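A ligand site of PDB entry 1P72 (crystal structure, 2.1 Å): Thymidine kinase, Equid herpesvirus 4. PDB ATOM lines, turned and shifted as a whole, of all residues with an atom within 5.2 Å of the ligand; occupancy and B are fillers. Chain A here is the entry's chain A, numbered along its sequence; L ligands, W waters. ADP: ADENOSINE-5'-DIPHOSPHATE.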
ATOM      1  N   VAL A  15      25.019  22.970 -16.646  1.00  0.00           N
ATOM      2  CA  VAL A  15      25.697  21.786 -17.179  1.00  0.00           C
ATOM      3  C   VAL A  15      26.018  21.972 -18.649  1.00  0.00           C
ATOM      4  O   VAL A  15      25.216  22.534 -19.419  1.00  0.00           O
ATOM      5  CB  VAL A  15      24.882  20.459 -16.935  1.00  0.00           C
ATOM      6  CG1 VAL A  15      25.732  19.213 -17.331  1.00  0.00           C
ATOM      7  CG2 VAL A  15      24.441  20.361 -15.479  1.00  0.00           C
ATOM      8  N   TYR A  16      27.205  21.526 -19.043  1.00  0.00           N
ATOM      9  CA  TYR A  16      27.539  21.575 -20.470  1.00  0.00           C
ATOM     10  C   TYR A  16      26.538  20.820 -21.340  1.00  0.00           C
ATOM     11  O   TYR A  16      26.018  19.774 -20.945  1.00  0.00           O
ATOM     12  CB  TYR A  16      28.956  21.080 -20.719  1.00  0.00           C
ATOM     13  CG  TYR A  16      29.203  19.626 -20.408  1.00  0.00           C
ATOM     14  CD1 TYR A  16      29.153  18.647 -21.422  1.00  0.00           C
ATOM     15  CD2 TYR A  16      29.543  19.213 -19.113  1.00  0.00           C
ATOM     16  CE1 TYR A  16      29.412  17.279 -21.123  1.00  0.00           C
ATOM     17  CE2 TYR A  16      29.806  17.878 -18.817  1.00  0.00           C
ATOM     18  CZ  TYR A  16      29.750  16.921 -19.811  1.00  0.00           C
ATOM     19  OH  TYR A  16      30.000  15.599 -19.476  1.00  0.00           O
ATOM     20  N   GLY A  17      26.246  21.364 -22.506  1.00  0.00           N
ATOM     21  CA  GLY A  17      25.317  20.688 -23.409  1.00  0.00           C
ATOM     22  C   GLY A  17      23.905  21.228 -23.472  1.00  0.00           C
ATOM     23  O   GLY A  17      23.175  20.909 -24.422  1.00  0.00           O
ATOM     24  N   ILE A  18      23.532  22.050 -22.495  1.00  0.00           N
ATOM     25  CA  ILE A  18      22.154  22.555 -22.416  1.00  0.00           C
ATOM     26  C   ILE A  18      21.839  23.640 -23.435  1.00  0.00           C
ATOM     27  O   ILE A  18      20.724  23.697 -23.928  1.00  0.00           O
ATOM     28  CB  ILE A  18      21.790  23.021 -20.967  1.00  0.00           C
ATOM     29  CG1 ILE A  18      21.639  21.809 -20.059  1.00  0.00           C
ATOM     30  CG2 ILE A  18      20.448  23.855 -20.948  1.00  0.00           C
ATOM     31  CD1 ILE A  18      21.485  22.088 -18.553  1.00  0.00           C
ATOM     32  N   GLY A  19      22.811  24.485 -23.774  1.00  0.00           N
ATOM     33  CA  GLY A  19      22.576  25.566 -24.742  1.00  0.00           C
ATOM     34  C   GLY A  19      22.960  26.957 -24.266  1.00  0.00           C
ATOM     35  O   GLY A  19      22.533  27.967 -24.830  1.00  0.00           O
ATOM     36  N   LYS A  20      23.764  27.008 -23.208  1.00  0.00           N
ATOM     37  CA  LYS A  20      24.173  28.264 -22.582  1.00  0.00           C
ATOM     38  C   LYS A  20      24.976  29.202 -23.524  1.00  0.00           C
ATOM     39  O   LYS A  20      24.652  30.383 -23.682  1.00  0.00           O
ATOM     40  CB  LYS A  20      24.976  27.892 -21.306  1.00  0.00           C
ATOM     41  CG  LYS A  20      25.988  28.936 -20.812  1.00  0.00           C
ATOM     42  CD  LYS A  20      26.815  28.364 -19.588  1.00  0.00           C
ATOM     43  CE  LYS A  20      27.605  27.091 -19.876  1.00  0.00           C
ATOM     44  NZ  LYS A  20      28.467  27.144 -21.103  1.00  0.00           N
ATOM     45  N   SER A  21      26.030  28.670 -24.129  1.00  0.00           N
ATOM     46  CA  SER A  21      26.938  29.482 -24.964  1.00  0.00           C
ATOM     47  C   SER A  21      26.213  30.010 -26.178  1.00  0.00           C
ATOM     48  O   SER A  21      26.388  31.179 -26.543  1.00  0.00           O
ATOM     49  CB  SER A  21      28.155  28.660 -25.396  1.00  0.00           C
ATOM     50  OG  SER A  21      29.008  28.463 -24.281  1.00  0.00           O
ATOM     51  N   THR A  22      25.394  29.165 -26.804  1.00  0.00           N
ATOM     52  CA  THR A  22      24.555  29.594 -27.924  1.00  0.00           C
ATOM     53  C   THR A  22      23.594  30.715 -27.507  1.00  0.00           C
ATOM     54  O   THR A  22      23.452  31.727 -28.210  1.00  0.00           O
ATOM     55  CB  THR A  22      23.767  28.380 -28.456  1.00  0.00           C
ATOM     56  OG1 THR A  22      24.696  27.393 -28.901  1.00  0.00           O
ATOM     57  CG2 THR A  22      22.956  28.738 -29.680  1.00  0.00           C
ATOM     58  N   THR A  23      22.928  30.525 -26.388  1.00  0.00           N
ATOM     59  CA  THR A  23      22.052  31.563 -25.848  1.00  0.00           C
ATOM     60  C   THR A  23      22.775  32.918 -25.623  1.00  0.00           C
ATOM     61  O   THR A  23      22.276  33.962 -26.059  1.00  0.00           O
ATOM     62  CB  THR A  23      21.427  31.078 -24.530  1.00  0.00           C
ATOM     63  OG1 THR A  23      20.683  29.875 -24.781  1.00  0.00           O
ATOM     64  CG2 THR A  23      20.385  32.116 -24.016  1.00  0.00           C
ATOM     65  N   ARG A  25      25.570  34.043 -26.982  1.00  0.00           N
ATOM     66  CA  ARG A  25      25.936  34.649 -28.263  1.00  0.00           C
ATOM     67  C   ARG A  25      24.744  35.350 -28.932  1.00  0.00           C
ATOM     68  O   ARG A  25      24.890  36.408 -29.492  1.00  0.00           O
ATOM     69  CB  ARG A  25      26.531  33.606 -29.228  1.00  0.00           C
ATOM     70  CG  ARG A  25      27.803  32.961 -28.709  1.00  0.00           C
ATOM     71  CD  ARG A  25      28.547  32.108 -29.731  1.00  0.00           C
ATOM     72  NE  ARG A  25      27.852  30.859 -30.010  1.00  0.00           N
ATOM     73  CZ  ARG A  25      28.218  29.656 -29.568  1.00  0.00           C
ATOM     74  NH1 ARG A  25      29.302  29.506 -28.822  1.00  0.00           N
ATOM     75  NH2 ARG A  25      27.511  28.602 -29.897  1.00  0.00           N
ATOM     76  N   ASP A 120      29.924  33.749 -19.684  1.00  0.00           N
ATOM     77  CA  ASP A 120      29.706  32.315 -19.866  1.00  0.00           C
ATOM     78  C   ASP A 120      30.335  31.614 -18.683  1.00  0.00           C
ATOM     79  O   ASP A 120      31.563  31.436 -18.647  1.00  0.00           O
ATOM     80  CB  ASP A 120      30.372  31.842 -21.159  1.00  0.00           C
ATOM     81  CG  ASP A 120      29.784  30.530 -21.671  1.00  0.00           C
ATOM     82  OD1 ASP A 120      29.746  29.538 -20.908  1.00  0.00           O
ATOM     83  OD2 ASP A 120      29.346  30.397 -22.808  1.00  0.00           O
ATOM     84  N   ARG A 121      29.477  31.238 -17.720  1.00  0.00           N
ATOM     85  CA  ARG A 121      29.842  30.706 -16.400  1.00  0.00           C
ATOM     86  C   ARG A 121      30.371  31.742 -15.417  1.00  0.00           C
ATOM     87  O   ARG A 121      31.019  32.696 -15.800  1.00  0.00           O
ATOM     88  CB  ARG A 121      30.849  29.533 -16.487  1.00  0.00           C
ATOM     89  CG  ARG A 121      30.443  28.431 -17.471  1.00  0.00           C
ATOM     90  CD  ARG A 121      31.366  27.199 -17.442  1.00  0.00           C
ATOM     91  NE  ARG A 121      30.814  26.107 -18.249  1.00  0.00           N
ATOM     92  CZ  ARG A 121      29.870  25.272 -17.830  1.00  0.00           C
ATOM     93  NH1 ARG A 121      29.305  25.431 -16.644  1.00  0.00           N
ATOM     94  NH2 ARG A 121      29.441  24.296 -18.621  1.00  0.00           N
ATOM     95  N   GLU A 170      16.087  16.121 -23.948  1.00  0.00           N
ATOM     96  CA  GLU A 170      16.504  17.131 -24.927  1.00  0.00           C
ATOM     97  C   GLU A 170      17.951  17.572 -24.656  1.00  0.00           C
ATOM     98  O   GLU A 170      18.713  17.835 -25.579  1.00  0.00           O
ATOM     99  CB  GLU A 170      15.535  18.336 -24.896  1.00  0.00           C
ATOM    100  CG  GLU A 170      15.913  19.544 -25.743  1.00  0.00           C
ATOM    101  CD  GLU A 170      15.971  19.259 -27.245  1.00  0.00           C
ATOM    102  OE1 GLU A 170      15.349  18.278 -27.708  1.00  0.00           O
ATOM    103  OE2 GLU A 170      16.660  20.016 -27.976  1.00  0.00           O
ATOM    104  N   ARG A 173      19.968  14.853 -26.200  1.00  0.00           N
ATOM    105  CA  ARG A 173      19.815  15.037 -27.637  1.00  0.00           C
ATOM    106  C   ARG A 173      20.721  16.135 -28.188  1.00  0.00           C
ATOM    107  O   ARG A 173      21.391  15.946 -29.208  1.00  0.00           O
ATOM    108  CB  ARG A 173      18.363  15.337 -27.993  1.00  0.00           C
ATOM    109  CG  ARG A 173      18.004  15.005 -29.447  1.00  0.00           C
ATOM    110  CD  ARG A 173      16.701  15.650 -29.924  1.00  0.00           C
ATOM    111  NE  ARG A 173      16.716  17.106 -29.795  1.00  0.00           N
ATOM    112  CZ  ARG A 173      17.381  17.944 -30.615  1.00  0.00           C
ATOM    113  NH1 ARG A 173      18.080  17.457 -31.652  1.00  0.00           N
ATOM    114  NH2 ARG A 173      17.342  19.259 -30.400  1.00  0.00           N
ATOM    115  N   ARG A 174      20.752  17.279 -27.512  1.00  0.00           N
ATOM    116  CA  ARG A 174      21.661  18.356 -27.896  1.00  0.00           C
ATOM    117  C   ARG A 174      23.128  17.911 -27.920  1.00  0.00           C
ATOM    118  O   ARG A 174      23.826  18.148 -28.907  1.00  0.00           O
ATOM    119  CB  ARG A 174      21.418  19.591 -27.048  1.00  0.00           C
ATOM    120  CG  ARG A 174      20.087  20.272 -27.410  1.00  0.00           C
ATOM    121  CD  ARG A 174      19.732  21.488 -26.577  1.00  0.00           C
ATOM    122  NE  ARG A 174      18.376  21.935 -26.878  1.00  0.00           N
ATOM    123  CZ  ARG A 174      17.825  23.049 -26.414  1.00  0.00           C
ATOM    124  NH1 ARG A 174      18.513  23.864 -25.616  1.00  0.00           N
ATOM    125  NH2 ARG A 174      16.590  23.356 -26.746  1.00  0.00           N
ATOM    126  N   LEU A 175      23.573  17.221 -26.873  1.00  0.00           N
ATOM    127  CA  LEU A 175      24.910  16.616 -26.881  1.00  0.00           C
ATOM    128  C   LEU A 175      25.149  15.611 -28.021  1.00  0.00           C
ATOM    129  O   LEU A 175      26.248  15.562 -28.591  1.00  0.00           O
ATOM    130  CB  LEU A 175      25.198  15.964 -25.550  1.00  0.00           C
ATOM    131  CG  LEU A 175      25.527  17.019 -24.502  1.00  0.00           C
ATOM    132  CD1 LEU A 175      25.547  16.422 -23.107  1.00  0.00           C
ATOM    133  CD2 LEU A 175      26.856  17.667 -24.872  1.00  0.00           C
ATOM    134  N   THR A 177      23.556  15.419 -31.183  1.00  0.00           N
ATOM    135  CA  THR A 177      23.643  16.076 -32.506  1.00  0.00           C
ATOM    136  C   THR A 177      25.077  16.496 -32.766  1.00  0.00           C
ATOM    137  O   THR A 177      25.652  16.227 -33.834  1.00  0.00           O
ATOM    138  CB  THR A 177      22.745  17.350 -32.607  1.00  0.00           C
ATOM    139  OG1 THR A 177      23.276  18.391 -31.764  1.00  0.00           O
ATOM    140  CG2 THR A 177      21.363  17.086 -32.071  1.00  0.00           C
ATOM    141  N   ARG A 178      25.649  17.155 -31.761  1.00  0.00           N
ATOM    142  CA  ARG A 178      26.969  17.738 -31.833  1.00  0.00           C
ATOM    143  C   ARG A 178      28.078  16.667 -31.880  1.00  0.00           C
ATOM    144  O   ARG A 178      29.067  16.841 -32.593  1.00  0.00           O
ATOM    145  CB  ARG A 178      27.168  18.690 -30.667  1.00  0.00           C
ATOM    146  CG  ARG A 178      28.397  19.542 -30.778  1.00  0.00           C
ATOM    147  CD  ARG A 178      29.226  19.555 -29.510  1.00  0.00           C
ATOM    148  NE  ARG A 178      29.277  20.909 -28.966  1.00  0.00           N
ATOM    149  CZ  ARG A 178      28.867  21.245 -27.756  1.00  0.00           C
ATOM    150  NH1 ARG A 178      28.364  20.321 -26.932  1.00  0.00           N
ATOM    151  NH2 ARG A 178      28.942  22.512 -27.361  1.00  0.00           N
ATOM    152  N   LEU A 290      15.714  26.376 -21.226  1.00  0.00           N
ATOM    153  CA  LEU A 290      16.239  26.575 -22.570  1.00  0.00           C
ATOM    154  C   LEU A 290      15.640  25.655 -23.651  1.00  0.00           C
ATOM    155  O   LEU A 290      16.329  25.278 -24.611  1.00  0.00           O
ATOM    156  CB  LEU A 290      17.793  26.481 -22.588  1.00  0.00           C
ATOM    157  CG  LEU A 290      18.665  27.445 -21.750  1.00  0.00           C
ATOM    158  CD1 LEU A 290      20.100  27.437 -22.248  1.00  0.00           C
ATOM    159  CD2 LEU A 290      18.142  28.871 -21.650  1.00  0.00           C
ATOM    160  N   GLY A 292      13.234  26.345 -25.816  1.00  0.00           N
ATOM    161  CA  GLY A 292      12.918  27.068 -27.044  1.00  0.00           C
ATOM    162  C   GLY A 292      14.089  27.144 -28.023  1.00  0.00           C
ATOM    163  O   GLY A 292      15.148  26.531 -27.787  1.00  0.00           O
ATOM    164  N   THR A 293      13.898  27.855 -29.140  1.00  0.00           N
ATOM    165  CA  THR A 293      14.969  28.121 -30.122  1.00  0.00           C
ATOM    166  C   THR A 293      16.021  29.030 -29.440  1.00  0.00           C
ATOM    167  O   THR A 293      15.738  29.579 -28.392  1.00  0.00           O
ATOM    168  CB  THR A 293      14.389  28.830 -31.393  1.00  0.00           C
ATOM    169  OG1 THR A 293      13.826  30.096 -31.013  1.00  0.00           O
ATOM    170  CG2 THR A 293      13.188  28.058 -31.993  1.00  0.00           C
ATOM    171  N   PRO A 294      17.237  29.155 -29.986  1.00  0.00           N
ATOM    172  CA  PRO A 294      18.209  30.124 -29.447  1.00  0.00           C
ATOM    173  C   PRO A 294      17.655  31.550 -29.306  1.00  0.00           C
ATOM    174  O   PRO A 294      17.919  32.175 -28.261  1.00  0.00           O
ATOM    175  CB  PRO A 294      19.354  30.059 -30.468  1.00  0.00           C
ATOM    176  CG  PRO A 294      19.312  28.612 -30.944  1.00  0.00           C
ATOM    177  CD  PRO A 294      17.822  28.361 -31.085  1.00  0.00           C
ATOM    178  N   CYS A 297      15.402  31.407 -26.271  1.00  0.00           N
ATOM    179  CA  CYS A 297      16.238  31.309 -25.058  1.00  0.00           C
ATOM    180  C   CYS A 297      16.833  32.652 -24.648  1.00  0.00           C
ATOM    181  O   CYS A 297      16.788  33.047 -23.455  1.00  0.00           O
ATOM    182  CB  CYS A 297      17.349  30.267 -25.271  1.00  0.00           C
ATOM    183  SG  CYS A 297      16.738  28.591 -25.488  1.00  0.00           S
HETATM  184  PB  ADP L   1      26.472  24.823 -23.418  1.00  0.00           P
HETATM  185  O1B ADP L   1      27.544  23.800 -23.137  1.00  0.00           O
HETATM  186  O2B ADP L   1      27.130  26.166 -23.577  1.00  0.00           O
HETATM  187  O3B ADP L   1      25.425  24.782 -22.326  1.00  0.00           O
HETATM  188  PA  ADP L   1      26.029  24.991 -26.220  1.00  0.00           P
HETATM  189  O1A ADP L   1      25.585  26.388 -26.509  1.00  0.00           O
HETATM  190  O2A ADP L   1      27.467  24.576 -26.453  1.00  0.00           O
HETATM  191  O3A ADP L   1      25.626  24.484 -24.749  1.00  0.00           O
HETATM  192  O5' ADP L   1      25.045  24.016 -27.027  1.00  0.00           O
HETATM  193  C5' ADP L   1      25.078  22.594 -26.892  1.00  0.00           C
HETATM  194  C4' ADP L   1      24.552  22.038 -28.206  1.00  0.00           C
HETATM  195  O4' ADP L   1      23.165  22.279 -28.349  1.00  0.00           O
HETATM  196  C3' ADP L   1      25.198  22.693 -29.417  1.00  0.00           C
HETATM  197  O3' ADP L   1      25.357  21.651 -30.370  1.00  0.00           O
HETATM  198  C2' ADP L   1      24.192  23.748 -29.881  1.00  0.00           C
HETATM  199  O2' ADP L   1      24.207  24.032 -31.287  1.00  0.00           O
HETATM  200  C1' ADP L   1      22.876  23.111 -29.469  1.00  0.00           C
HETATM  201  N9  ADP L   1      21.916  24.136 -29.025  1.00  0.00           N
HETATM  202  C8  ADP L   1      22.206  25.229 -28.301  1.00  0.00           C
HETATM  203  N7  ADP L   1      21.062  25.900 -28.084  1.00  0.00           N
HETATM  204  C5  ADP L   1      20.066  25.210 -28.658  1.00  0.00           C
HETATM  205  C6  ADP L   1      18.600  25.450 -28.735  1.00  0.00           C
HETATM  206  N6  ADP L   1      18.103  26.480 -28.191  1.00  0.00           N
HETATM  207  N1  ADP L   1      17.819  24.576 -29.380  1.00  0.00           N
HETATM  208  C2  ADP L   1      18.405  23.419 -30.018  1.00  0.00           C
HETATM  209  N3  ADP L   1      19.836  23.205 -29.913  1.00  0.00           N
HETATM  210  C4  ADP L   1      20.608  24.094 -29.250  1.00  0.00           C
HETATM  211  O   HOH W   1      29.499  25.527 -25.233  1.00  0.00           O
HETATM  212  O   HOH W   2      29.486  24.366 -21.424  1.00  0.00           O
HETATM  213  O   HOH W   3      15.479  24.588 -30.727  1.00  0.00           O
HETATM  214  O   HOH W   4      20.112  28.496 -27.294  1.00  0.00           O
HETATM  215  O   HOH W   5      24.460  25.038 -19.783  1.00  0.00           O
HETATM  216  O   HOH W   6      28.762  22.278 -24.963  1.00  0.00           O
HETATM  217  O   HOH W   7      20.698  21.020 -31.470  1.00  0.00           O
HETATM  218  O   HOH W   8      28.321  26.602 -28.837  1.00  0.00           O
HETATM  219  O   HOH W   9      27.451  22.140 -33.003  1.00  0.00           O
HETATM  220  O   HOH W  10      25.078  26.609 -31.578  1.00  0.00           O
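OD1 of Asp 120 lies within salt-bridge range of NZ of Lys 20 (2.7 Å).
O of Gly 19 lies within hydrogen-bond range of OG1 of Thr 23, at 2.7 Å.
O of Gly 292 lies within hydrogen-bond range of SG of Cys 297 (3.5 Å).
The backbone carbonyl oxygen (O) of Ile 18 lies within hydrogen-bond range of the guanidinium group (NH1) of Arg 174 (2.8 Å).
The backbone carbonyl oxygen (O) of Arg 174 is in hydrogen-bond range of the side-chain hydroxyl (OG1) of Thr 177, 2.9 Å away.
The backbone carbonyl oxygen of Leu 290 is in hydrogen-bond range of the guanidinium group of Arg 174 (2.8 Å).
NE of Arg 174 is in salt-bridge range of OE2 of Glu 170 (2.8 Å).
The backbone carbonyl oxygen (O) of Leu 290 is in hydrogen-bond range of the side-chain sulfur (SG) of Cys 297 (3.5 Å).
The backbone nitrogen (N) of Pro 294 sits close to a nitrogen (N6) of the ligand, at 3.3 Å.
Merely in contact with the ligand: Val 15 (3.7 Å), Tyr 16 (3.5 Å) and Thr 293 (3.5 Å).
Hydrophobic or aromatic side chains within 4 Å of the ligand: Tyr 16 and Pro 294.
Along chain A the residues within 4 Å of the ligand span positions 15 to 297.
The nearest printed residue that does not touch the ligand is Thr 177 (4.1 Å).
An oxygen (O2A) of the ligand is in salt-bridge range of the guanidinium group (NH2) of Arg 178.
An oxygen (O1A) of the ligand sits at hydrogen-bond distance from the backbone NH (N) of Thr 22 (2.8 Å).
The side-chain hydroxyl (OG1) of Thr 22 lies within hydrogen-bond range of an oxygen (O1A) of the ligand (2.7 Å).
The backbone NH (N) of Ser 21 sits at hydrogen-bond distance from an oxygen (O2B) of the ligand (2.8 Å).
The side-chain hydroxyl (OG) of Ser 21 is in hydrogen-bond range of an oxygen (O2B) of the ligand (3.0 Å).
O1B of the ligand is in hydrogen-bond range of N of Gly 17, 2.8 Å away.
N of Lys 20 lies within hydrogen-bond range of O3B of the ligand.
O2B of the ligand lies within salt-bridge range of NZ of Lys 20 (3.0 Å).
O3A of the ligand sits at hydrogen-bond distance from N of Gly 19 (3.0 Å).
The backbone carbonyl oxygen of Gly 292 sits at hydrogen-bond distance from a nitrogen (N6) of the ligand, at 3.0 Å.
The guanidinium group of Arg 174 is in hydrogen-bond range of a nitrogen (N1) of the ligand, 3.2 Å away.
An oxygen (O3B) of the ligand lies within hydrogen-bond range of the backbone NH (N) of Ile 18 (3.3 Å).
A nitrogen (N6) of the ligand is in hydrogen-bond range of the side-chain sulfur (SG) of Cys 297 (3.7 Å).
Water W1 lies within hydrogen-bond range of O2A of the ligand and OG of Ser 21.
Water W2 lies within hydrogen-bond range of an oxygen (O1B) of the ligand (2.7 Å), the guanidinium group of Arg 121 (2.8 Å) and the side-chain amino group of Lys 20 (3.0 Å).
Water W5 bridges the backbone carbonyl oxygen (O) of Val 15 (2.6 Å) and an oxygen (O3B) of the ligand (2.7 Å).
Water W10 bridges an oxygen (O2') of the ligand (2.7 Å) and the side-chain hydroxyl (OG1) of Thr 22 (2.8 Å).
Water W4 lies within hydrogen-bond range of a nitrogen (N7) of the ligand (2.9 Å), the side-chain hydroxyl (OG1) of Thr 23 (2.9 Å) and the backbone carbonyl oxygen (O) of Gly 19 (3.5 Å).
Water W8 bridges NH2 of Arg 25 (2.4 Å) and O2A of the ligand (3.2 Å).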
